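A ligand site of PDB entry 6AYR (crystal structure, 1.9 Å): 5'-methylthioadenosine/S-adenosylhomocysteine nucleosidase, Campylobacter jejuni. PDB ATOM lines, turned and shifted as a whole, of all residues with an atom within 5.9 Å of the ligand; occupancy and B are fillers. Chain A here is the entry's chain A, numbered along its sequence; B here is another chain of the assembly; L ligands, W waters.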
ATOM      1  N   ALA A  18      23.748  28.493 -11.325  1.00  0.00           N
ATOM      2  CA  ALA A  18      23.738  28.358 -12.788  1.00  0.00           C
ATOM      3  C   ALA A  18      22.382  28.768 -13.387  1.00  0.00           C
ATOM      4  O   ALA A  18      22.340  29.375 -14.436  1.00  0.00           O
ATOM      5  CB  ALA A  18      24.059  26.929 -13.175  1.00  0.00           C
ATOM      6  N   MET A  19      21.289  28.421 -12.691  1.00  0.00           N
ATOM      7  CA  MET A  19      19.920  28.574 -13.197  1.00  0.00           C
ATOM      8  C   MET A  19      19.107  29.517 -12.330  1.00  0.00           C
ATOM      9  O   MET A  19      19.416  29.705 -11.152  1.00  0.00           O
ATOM     10  CB  MET A  19      19.212  27.212 -13.250  1.00  0.00           C
ATOM     11  CG  MET A  19      19.850  26.227 -14.209  1.00  0.00           C
ATOM     12  SD  MET A  19      19.099  24.568 -14.252  1.00  0.00           S
ATOM     13  CE  MET A  19      17.594  24.950 -15.151  1.00  0.00           C
ATOM     14  N   GLU A  22      17.946  28.325  -8.934  1.00  0.00           N
ATOM     15  CA  GLU A  22      18.946  28.240  -7.847  1.00  0.00           C
ATOM     16  C   GLU A  22      19.168  29.558  -7.099  1.00  0.00           C
ATOM     17  O   GLU A  22      19.713  29.562  -6.004  1.00  0.00           O
ATOM     18  CB  GLU A  22      20.260  27.678  -8.405  1.00  0.00           C
ATOM     19  CG  GLU A  22      20.108  26.264  -8.996  1.00  0.00           C
ATOM     20  CD  GLU A  22      21.235  25.826  -9.935  1.00  0.00           C
ATOM     21  OE1 GLU A  22      21.791  26.666 -10.663  1.00  0.00           O
ATOM     22  OE2 GLU A  22      21.537  24.615  -9.977  1.00  0.00           O
ATOM     23  N   ILE A  60      23.911  27.985 -17.883  1.00  0.00           N
ATOM     24  CA  ILE A  60      24.458  26.640 -17.655  1.00  0.00           C
ATOM     25  C   ILE A  60      25.865  26.465 -18.226  1.00  0.00           C
ATOM     26  O   ILE A  60      26.171  26.948 -19.322  1.00  0.00           O
ATOM     27  CB  ILE A  60      23.507  25.561 -18.220  1.00  0.00           C
ATOM     28  CG1 ILE A  60      22.195  25.589 -17.433  1.00  0.00           C
ATOM     29  CG2 ILE A  60      24.142  24.169 -18.168  1.00  0.00           C
ATOM     30  CD1 ILE A  60      21.038  24.866 -18.107  1.00  0.00           C
ATOM     31  N   GLY A  61      26.718  25.795 -17.459  1.00  0.00           N
ATOM     32  CA  GLY A  61      27.994  25.302 -17.966  1.00  0.00           C
ATOM     33  C   GLY A  61      29.259  26.015 -17.506  1.00  0.00           C
ATOM     34  O   GLY A  61      29.213  26.999 -16.750  1.00  0.00           O
ATOM     35  N   VAL A  86      22.090  22.640  -7.631  1.00  0.00           N
ATOM     36  CA  VAL A  86      21.739  21.224  -7.553  1.00  0.00           C
ATOM     37  C   VAL A  86      22.813  20.381  -8.248  1.00  0.00           C
ATOM     38  O   VAL A  86      23.722  20.922  -8.871  1.00  0.00           O
ATOM     39  CB  VAL A  86      20.320  20.929  -8.118  1.00  0.00           C
ATOM     40  CG1 VAL A  86      19.273  21.683  -7.296  1.00  0.00           C
ATOM     41  CG2 VAL A  86      20.173  21.269  -9.606  1.00  0.00           C
ATOM     42  N   ALA A  87      22.706  19.067  -8.127  1.00  0.00           N
ATOM     43  CA  ALA A  87      23.700  18.163  -8.692  1.00  0.00           C
ATOM     44  C   ALA A  87      23.142  16.767  -8.921  1.00  0.00           C
ATOM     45  O   ALA A  87      22.094  16.427  -8.382  1.00  0.00           O
ATOM     46  CB  ALA A  87      24.949  18.098  -7.795  1.00  0.00           C
ATOM     47  N   GLY A  88      23.852  15.977  -9.714  1.00  0.00           N
ATOM     48  CA  GLY A  88      23.549  14.560  -9.920  1.00  0.00           C
ATOM     49  C   GLY A  88      24.357  13.712  -8.962  1.00  0.00           C
ATOM     50  O   GLY A  88      25.569  13.878  -8.869  1.00  0.00           O
ATOM     51  N   TYR A 108      36.021  16.523 -15.564  1.00  0.00           N
ATOM     52  CA  TYR A 108      36.117  15.176 -16.180  1.00  0.00           C
ATOM     53  C   TYR A 108      36.231  15.177 -17.719  1.00  0.00           C
ATOM     54  O   TYR A 108      36.562  14.145 -18.309  1.00  0.00           O
ATOM     55  CB  TYR A 108      34.975  14.246 -15.740  1.00  0.00           C
ATOM     56  CG  TYR A 108      33.579  14.644 -16.220  1.00  0.00           C
ATOM     57  CD1 TYR A 108      33.150  14.379 -17.508  1.00  0.00           C
ATOM     58  CD2 TYR A 108      32.702  15.320 -15.365  1.00  0.00           C
ATOM     59  CE1 TYR A 108      31.891  14.777 -17.947  1.00  0.00           C
ATOM     60  CE2 TYR A 108      31.445  15.711 -15.791  1.00  0.00           C
ATOM     61  CZ  TYR A 108      31.035  15.423 -17.071  1.00  0.00           C
ATOM     62  OH  TYR A 108      29.782  15.838 -17.501  1.00  0.00           O
ATOM     63  N   GLY A 158      31.634  18.905 -15.671  1.00  0.00           N
ATOM     64  CA  GLY A 158      31.803  18.851 -17.118  1.00  0.00           C
ATOM     65  C   GLY A 158      30.583  19.416 -17.794  1.00  0.00           C
ATOM     66  O   GLY A 158      29.587  19.696 -17.139  1.00  0.00           O
ATOM     67  N   GLU A 160      28.321  18.223 -19.848  1.00  0.00           N
ATOM     68  CA  GLU A 160      27.290  17.289 -20.273  1.00  0.00           C
ATOM     69  C   GLU A 160      26.341  17.043 -19.096  1.00  0.00           C
ATOM     70  O   GLU A 160      26.790  16.942 -17.959  1.00  0.00           O
ATOM     71  CB  GLU A 160      27.950  15.986 -20.704  1.00  0.00           C
ATOM     72  CG  GLU A 160      26.985  14.932 -21.262  1.00  0.00           C
ATOM     73  CD  GLU A 160      27.679  13.625 -21.642  1.00  0.00           C
ATOM     74  OE1 GLU A 160      28.867  13.684 -22.056  1.00  0.00           O
ATOM     75  OE2 GLU A 160      27.049  12.534 -21.519  1.00  0.00           O
ATOM     76  N   PHE A 161      25.040  16.982 -19.372  1.00  0.00           N
ATOM     77  CA  PHE A 161      24.071  16.431 -18.414  1.00  0.00           C
ATOM     78  C   PHE A 161      24.204  14.912 -18.429  1.00  0.00           C
ATOM     79  O   PHE A 161      24.001  14.276 -19.456  1.00  0.00           O
ATOM     80  CB  PHE A 161      22.634  16.837 -18.769  1.00  0.00           C
ATOM     81  CG  PHE A 161      21.632  16.410 -17.729  1.00  0.00           C
ATOM     82  CD1 PHE A 161      21.514  17.098 -16.535  1.00  0.00           C
ATOM     83  CD2 PHE A 161      20.843  15.266 -17.918  1.00  0.00           C
ATOM     84  CE1 PHE A 161      20.619  16.690 -15.562  1.00  0.00           C
ATOM     85  CE2 PHE A 161      19.952  14.845 -16.945  1.00  0.00           C
ATOM     86  CZ  PHE A 161      19.846  15.559 -15.763  1.00  0.00           C
ATOM     87  N   ILE A 162      24.562  14.341 -17.284  1.00  0.00           N
ATOM     88  CA  ILE A 162      24.892  12.902 -17.180  1.00  0.00           C
ATOM     89  C   ILE A 162      23.626  12.133 -16.848  1.00  0.00           C
ATOM     90  O   ILE A 162      23.014  12.391 -15.803  1.00  0.00           O
ATOM     91  CB  ILE A 162      25.968  12.626 -16.096  1.00  0.00           C
ATOM     92  CG1 ILE A 162      27.246  13.422 -16.374  1.00  0.00           C
ATOM     93  CG2 ILE A 162      26.254  11.128 -15.963  1.00  0.00           C
ATOM     94  CD1 ILE A 162      27.952  13.052 -17.656  1.00  0.00           C
ATOM     95  N   CYS A 163      23.230  11.204 -17.723  1.00  0.00           N
ATOM     96  CA  CYS A 163      22.012  10.405 -17.527  1.00  0.00           C
ATOM     97  C   CYS A 163      22.174   9.020 -18.115  1.00  0.00           C
ATOM     98  O   CYS A 163      21.318   8.522 -18.863  1.00  0.00           O
ATOM     99  CB  CYS A 163      20.803  11.131 -18.129  1.00  0.00           C
ATOM    100  SG  CYS A 163      21.040  11.678 -19.825  1.00  0.00           S
ATOM    101  N   CYS A 180      28.097  14.887  -9.719  1.00  0.00           N
ATOM    102  CA  CYS A 180      28.495  15.540 -10.934  1.00  0.00           C
ATOM    103  C   CYS A 180      27.665  16.793 -11.130  1.00  0.00           C
ATOM    104  O   CYS A 180      26.544  16.890 -10.629  1.00  0.00           O
ATOM    105  CB  CYS A 180      28.345  14.631 -12.154  1.00  0.00           C
ATOM    106  SG  CYS A 180      26.660  14.264 -12.670  1.00  0.00           S
ATOM    107  N   GLU A 181      28.239  17.729 -11.873  1.00  0.00           N
ATOM    108  CA  GLU A 181      27.526  18.953 -12.206  1.00  0.00           C
ATOM    109  C   GLU A 181      28.291  19.704 -13.296  1.00  0.00           C
ATOM    110  O   GLU A 181      29.193  19.126 -13.903  1.00  0.00           O
ATOM    111  CB  GLU A 181      27.157  19.700 -10.908  1.00  0.00           C
ATOM    112  CG  GLU A 181      28.249  19.897  -9.926  1.00  0.00           C
ATOM    113  CD  GLU A 181      29.222  21.025 -10.176  1.00  0.00           C
ATOM    114  OE1 GLU A 181      29.941  21.011 -11.194  1.00  0.00           O
ATOM    115  OE2 GLU A 181      29.533  21.525  -9.099  1.00  0.00           O
ATOM    116  N   MET A 182      27.895  20.927 -13.644  1.00  0.00           N
ATOM    117  CA  MET A 182      28.410  21.575 -14.860  1.00  0.00           C
ATOM    118  C   MET A 182      29.082  22.933 -14.617  1.00  0.00           C
ATOM    119  O   MET A 182      29.459  23.603 -15.575  1.00  0.00           O
ATOM    120  CB  MET A 182      27.277  21.684 -15.902  1.00  0.00           C
ATOM    121  CG  MET A 182      26.579  20.346 -16.236  1.00  0.00           C
ATOM    122  SD  MET A 182      25.142  20.445 -17.319  1.00  0.00           S
ATOM    123  CE  MET A 182      25.845  20.891 -18.916  1.00  0.00           C
ATOM    124  N   GLU A 183      29.238  23.331 -13.351  1.00  0.00           N
ATOM    125  CA  GLU A 183      29.814  24.651 -13.012  1.00  0.00           C
ATOM    126  C   GLU A 183      30.854  24.713 -11.871  1.00  0.00           C
ATOM    127  O   GLU A 183      31.509  25.746 -11.695  1.00  0.00           O
ATOM    128  CB  GLU A 183      28.700  25.635 -12.697  1.00  0.00           C
ATOM    129  CG  GLU A 183      27.659  25.789 -13.798  1.00  0.00           C
ATOM    130  CD  GLU A 183      26.585  24.709 -13.843  1.00  0.00           C
ATOM    131  OE1 GLU A 183      26.389  23.935 -12.876  1.00  0.00           O
ATOM    132  OE2 GLU A 183      25.882  24.654 -14.866  1.00  0.00           O
ATOM    133  N   ARG A 202      25.861  21.844  -3.135  1.00  0.00           N
ATOM    134  CA  ARG A 202      24.900  21.273  -4.058  1.00  0.00           C
ATOM    135  C   ARG A 202      23.890  20.388  -3.315  1.00  0.00           C
ATOM    136  O   ARG A 202      24.279  19.611  -2.454  1.00  0.00           O
ATOM    137  CB  ARG A 202      25.609  20.444  -5.117  1.00  0.00           C
ATOM    138  CG  ARG A 202      26.613  21.201  -5.972  1.00  0.00           C
ATOM    139  CD  ARG A 202      25.922  22.206  -6.880  1.00  0.00           C
ATOM    140  NE  ARG A 202      26.823  22.720  -7.925  1.00  0.00           N
ATOM    141  CZ  ARG A 202      26.458  23.206  -9.109  1.00  0.00           C
ATOM    142  NH1 ARG A 202      25.182  23.219  -9.501  1.00  0.00           N
ATOM    143  NH2 ARG A 202      27.388  23.648  -9.944  1.00  0.00           N
ATOM    144  N   SER A 205      19.385  16.714  -7.147  1.00  0.00           N
ATOM    145  CA  SER A 205      18.120  16.744  -7.898  1.00  0.00           C
ATOM    146  C   SER A 205      17.805  15.426  -8.603  1.00  0.00           C
ATOM    147  O   SER A 205      16.673  15.233  -9.064  1.00  0.00           O
ATOM    148  CB  SER A 205      18.171  17.850  -8.946  1.00  0.00           C
ATOM    149  OG  SER A 205      19.291  17.677  -9.800  1.00  0.00           O
ATOM    150  N   ASP A 206      18.798  14.530  -8.706  1.00  0.00           N
ATOM    151  CA  ASP A 206      18.666  13.271  -9.448  1.00  0.00           C
ATOM    152  C   ASP A 206      19.866  12.370  -9.139  1.00  0.00           C
ATOM    153  O   ASP A 206      20.753  12.745  -8.358  1.00  0.00           O
ATOM    154  CB  ASP A 206      18.547  13.547 -10.944  1.00  0.00           C
ATOM    155  CG  ASP A 206      19.765  14.269 -11.517  1.00  0.00           C
ATOM    156  OD1 ASP A 206      20.805  13.604 -11.733  1.00  0.00           O
ATOM    157  OD2 ASP A 206      19.686  15.500 -11.736  1.00  0.00           O
ATOM    158  N   LYS A 207      19.882  11.168  -9.729  1.00  0.00           N
ATOM    159  CA  LYS A 207      20.958  10.181  -9.509  1.00  0.00           C
ATOM    160  C   LYS A 207      21.803   9.902 -10.765  1.00  0.00           C
ATOM    161  O   LYS A 207      22.566   8.931 -10.793  1.00  0.00           O
ATOM    162  CB  LYS A 207      20.370   8.876  -8.958  1.00  0.00           C
ATOM    163  CG  LYS A 207      19.626   9.077  -7.644  1.00  0.00           C
ATOM    164  CD  LYS A 207      19.505   7.775  -6.877  1.00  0.00           C
ATOM    165  CE  LYS A 207      18.711   7.982  -5.586  1.00  0.00           C
ATOM    166  NZ  LYS A 207      19.057   6.954  -4.575  1.00  0.00           N
ATOM    167  N   ALA A 208      21.658  10.744 -11.784  1.00  0.00           N
ATOM    168  CA  ALA A 208      22.576  10.764 -12.937  1.00  0.00           C
ATOM    169  C   ALA A 208      22.646   9.459 -13.754  1.00  0.00           C
ATOM    170  O   ALA A 208      23.641   9.201 -14.404  1.00  0.00           O
ATOM    171  CB  ALA A 208      23.966  11.168 -12.470  1.00  0.00           C
ATOM    172  N   ALA A 212      17.353  10.349 -15.416  1.00  0.00           N
ATOM    173  CA  ALA A 212      17.801  11.459 -14.560  1.00  0.00           C
ATOM    174  C   ALA A 212      17.175  12.785 -14.993  1.00  0.00           C
ATOM    175  O   ALA A 212      16.888  13.632 -14.146  1.00  0.00           O
ATOM    176  CB  ALA A 212      19.319  11.583 -14.577  1.00  0.00           C
ATOM    177  N   PHE A 216      15.305  15.263 -12.545  1.00  0.00           N
ATOM    178  CA  PHE A 216      15.773  16.636 -12.505  1.00  0.00           C
ATOM    179  C   PHE A 216      14.591  17.581 -12.572  1.00  0.00           C
ATOM    180  O   PHE A 216      14.449  18.423 -11.680  1.00  0.00           O
ATOM    181  CB  PHE A 216      16.762  16.955 -13.646  1.00  0.00           C
ATOM    182  CG  PHE A 216      17.091  18.423 -13.740  1.00  0.00           C
ATOM    183  CD1 PHE A 216      18.078  18.957 -12.947  1.00  0.00           C
ATOM    184  CD2 PHE A 216      16.361  19.268 -14.563  1.00  0.00           C
ATOM    185  CE1 PHE A 216      18.388  20.308 -13.007  1.00  0.00           C
ATOM    186  CE2 PHE A 216      16.631  20.628 -14.613  1.00  0.00           C
ATOM    187  CZ  PHE A 216      17.658  21.152 -13.830  1.00  0.00           C
ATOM    188  N   ASP A 217      13.743  17.449 -13.596  1.00  0.00           N
ATOM    189  CA  ASP A 217      12.575  18.339 -13.769  1.00  0.00           C
ATOM    190  C   ASP A 217      11.650  18.309 -12.546  1.00  0.00           C
ATOM    191  O   ASP A 217      11.121  19.350 -12.157  1.00  0.00           O
ATOM    192  CB  ASP A 217      11.755  17.999 -15.027  1.00  0.00           C
ATOM    193  CG  ASP A 217      12.421  18.464 -16.340  1.00  0.00           C
ATOM    194  OD1 ASP A 217      13.038  19.566 -16.406  1.00  0.00           O
ATOM    195  OD2 ASP A 217      12.282  17.723 -17.345  1.00  0.00           O
ATOM    196  N   ILE B 112      23.164  19.410 -23.383  1.00  0.00           N
ATOM    197  CA  ILE B 112      21.965  19.133 -22.609  1.00  0.00           C
ATOM    198  C   ILE B 112      20.907  18.546 -23.546  1.00  0.00           C
ATOM    199  O   ILE B 112      19.699  18.784 -23.371  1.00  0.00           O
ATOM    200  CB  ILE B 112      21.449  20.381 -21.852  1.00  0.00           C
ATOM    201  CG1 ILE B 112      21.119  21.534 -22.794  1.00  0.00           C
ATOM    202  CG2 ILE B 112      22.481  20.826 -20.829  1.00  0.00           C
ATOM    203  CD1 ILE B 112      20.331  22.641 -22.124  1.00  0.00           C
ATOM    204  N   PHE B 115      17.384  16.959 -22.738  1.00  0.00           N
ATOM    205  CA  PHE B 115      16.155  17.755 -22.621  1.00  0.00           C
ATOM    206  C   PHE B 115      15.559  18.180 -23.983  1.00  0.00           C
ATOM    207  O   PHE B 115      14.679  19.038 -24.021  1.00  0.00           O
ATOM    208  CB  PHE B 115      16.407  18.972 -21.722  1.00  0.00           C
ATOM    209  CG  PHE B 115      16.773  18.606 -20.316  1.00  0.00           C
ATOM    210  CD1 PHE B 115      15.776  18.328 -19.363  1.00  0.00           C
ATOM    211  CD2 PHE B 115      18.108  18.471 -19.934  1.00  0.00           C
ATOM    212  CE1 PHE B 115      16.113  17.960 -18.069  1.00  0.00           C
ATOM    213  CE2 PHE B 115      18.441  18.116 -18.640  1.00  0.00           C
ATOM    214  CZ  PHE B 115      17.445  17.854 -17.695  1.00  0.00           C
ATOM    215  N   HIS B 117      17.103  19.708 -26.582  1.00  0.00           N
ATOM    216  CA  HIS B 117      17.713  20.902 -27.208  1.00  0.00           C
ATOM    217  C   HIS B 117      18.828  20.414 -28.182  1.00  0.00           C
ATOM    218  O   HIS B 117      19.367  19.312 -28.028  1.00  0.00           O
ATOM    219  CB  HIS B 117      18.323  21.857 -26.190  1.00  0.00           C
ATOM    220  CG  HIS B 117      17.328  22.510 -25.276  1.00  0.00           C
ATOM    221  ND1 HIS B 117      16.480  23.525 -25.686  1.00  0.00           N
ATOM    222  CD2 HIS B 117      17.088  22.340 -23.963  1.00  0.00           C
ATOM    223  CE1 HIS B 117      15.737  23.926 -24.668  1.00  0.00           C
ATOM    224  NE2 HIS B 117      16.087  23.212 -23.603  1.00  0.00           N
ATOM    225  N   PRO B 123      19.979  27.485 -22.550  1.00  0.00           N
ATOM    226  CA  PRO B 123      19.064  28.637 -22.516  1.00  0.00           C
ATOM    227  C   PRO B 123      19.752  29.972 -22.191  1.00  0.00           C
ATOM    228  O   PRO B 123      20.680  30.011 -21.384  1.00  0.00           O
ATOM    229  CB  PRO B 123      18.059  28.261 -21.414  1.00  0.00           C
ATOM    230  CG  PRO B 123      18.046  26.784 -21.454  1.00  0.00           C
ATOM    231  CD  PRO B 123      19.501  26.410 -21.653  1.00  0.00           C
HETATM  232  C1  LIG L   1      25.009  17.168 -14.881  1.00  0.00           C
HETATM  233  C2  LIG L   1      22.971  16.866 -13.024  1.00  0.00           C
HETATM  234  C3  LIG L   1      23.731  18.110 -13.190  1.00  0.00           C
HETATM  235  C4  LIG L   1      22.154  18.345 -11.593  1.00  0.00           C
HETATM  236  O1  LIG L   1      23.067  23.765 -14.436  1.00  0.00           O
HETATM  237  C5  LIG L   1      23.065  22.439 -14.955  1.00  0.00           C
HETATM  238  C6  LIG L   1      21.692  21.849 -14.737  1.00  0.00           C
HETATM  239  C7  LIG L   1      21.406  20.563 -15.500  1.00  0.00           C
HETATM  240  S1  LIG L   1      21.047  20.885 -17.193  1.00  0.00           S
HETATM  241  C8  LIG L   1      19.348  21.379 -17.124  1.00  0.00           C
HETATM  242  C9  LIG L   1      18.849  21.806 -18.488  1.00  0.00           C
HETATM  243  C10 LIG L   1      17.339  21.990 -18.454  1.00  0.00           C
HETATM  244  C11 LIG L   1      16.845  22.440 -19.821  1.00  0.00           C
HETATM  245  C12 LIG L   1      21.699  21.597 -13.231  1.00  0.00           C
HETATM  246  N1  LIG L   1      23.123  21.573 -12.830  1.00  0.00           N
HETATM  247  C13 LIG L   1      23.962  21.627 -14.061  1.00  0.00           C
HETATM  248  C14 LIG L   1      23.515  20.515 -11.907  1.00  0.00           C
HETATM  249  N2  LIG L   1      22.066  17.065 -12.050  1.00  0.00           N
HETATM  250  C15 LIG L   1      23.385  15.733 -13.908  1.00  0.00           C
HETATM  251  N3  LIG L   1      22.790  14.527 -13.862  1.00  0.00           N
HETATM  252  N4  LIG L   1      24.712  18.227 -14.118  1.00  0.00           N
HETATM  253  C16 LIG L   1      23.154  19.079 -12.240  1.00  0.00           C
HETATM  254  N5  LIG L   1      24.382  15.959 -14.784  1.00  0.00           N
HETATM  255  O   HOH W   1      28.292  16.906 -15.518  1.00  0.00           O
HETATM  256  O   HOH W   2      23.470  23.871 -11.504  1.00  0.00           O
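CB of Ala 18 touches O1 of the ligand, 3.5 Å away.
Met 19 touches the ligand (SD to C6, 3.8 Å).
CG1 of Ile 60 touches O1 of the ligand, 3.6 Å away.
Val 86 touches the ligand.
Ala 87 touches the ligand (C to C4, 3.3 Å).
Glu 160 touches the ligand (O to C1, 3.6 Å).
Phe 161 touches the ligand (CE1 to C15, 3.4 Å).
Glu 181 touches the ligand (CA to N4, 3.5 Å).
CG of Met 182 touches N4 of the ligand (3.5 Å).
Arg 202 touches the ligand.
OG of Ser 205 touches C4 of the ligand (3.4 Å).
Ala 208 touches the ligand.
CE1 of Phe 216 touches C12 of the ligand (3.6 Å).
Ile 112 of chain B touches the ligand (CG2 to S1, 3.9 Å).
CD2 of Phe 115 of chain B touches C9 of the ligand, 3.7 Å away.
NE2 of His 117 of chain B touches C11 of the ligand, 3.9 Å away.
21 residues have an atom within 4 Å of the ligand: Ala 18, Met 19, Ile 60, Val 86, Ala 87, Gly 88, Glu 160, Phe 161, Ile 162, Cys 180, Glu 181, Met 182, Glu 183, Arg 202, Ser 205, Asp 206, Ala 208, Phe 216, Ile 112 of chain B, Phe 115 of chain B and His 117 of chain B.
OD2 of Asp 206 sits at hydrogen-bond distance from N2 of the ligand.
The backbone NH (N) of Ile 162 sits at hydrogen-bond distance from a nitrogen (N5) of the ligand (3.0 Å).
The backbone carbonyl oxygen (O) of Ile 162 sits at hydrogen-bond distance from a nitrogen (N3) of the ligand (2.9 Å).
An oxygen (O1) of the ligand is in hydrogen-bond range of the side-chain carboxylate of Glu 183.
N2 of the ligand sits close to N of Gly 88, at 3.1 Å.
SG of Cys 180 lies within hydrogen-bond range of N5 of the ligand.
Water W2 lies within hydrogen-bond range of the side-chain carboxylate (OE2) of Glu 22 (2.6 Å), the guanidinium group (NH1) of Arg 202 (2.7 Å), an oxygen (O1) of the ligand (3.0 Å) and the side-chain carboxylate (OE1) of Glu 183 (3.2 Å).
OD2 of Asp 206 is in hydrogen-bond range of OG of Ser 205.
The backbone NH (N) of Glu 183 lies within hydrogen-bond range of the side-chain carboxylate (OE1) of Glu 181 (3.2 Å).
The side-chain carboxylate (OE1) of Glu 183 lies within salt-bridge range of the guanidinium group (NH2) of Arg 202.
The guanidinium group of Arg 202 is in salt-bridge range of the side-chain carboxylate of Glu 181 (3.1 Å).
The backbone NH (N) of Gly 158 is in hydrogen-bond range of the backbone carbonyl oxygen (O) of Glu 181, 3.0 Å away.
The side-chain carboxylate (OE1) of Glu 22 sits at hydrogen-bond distance from the backbone NH (N) of Ala 18 (2.8 Å).
The side-chain carboxylate (OE1) of Glu 22 sits at hydrogen-bond distance from the backbone NH (N) of Met 19.
OE2 of Glu 22 is in salt-bridge range of NH1 of Arg 202 (3.9 Å).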
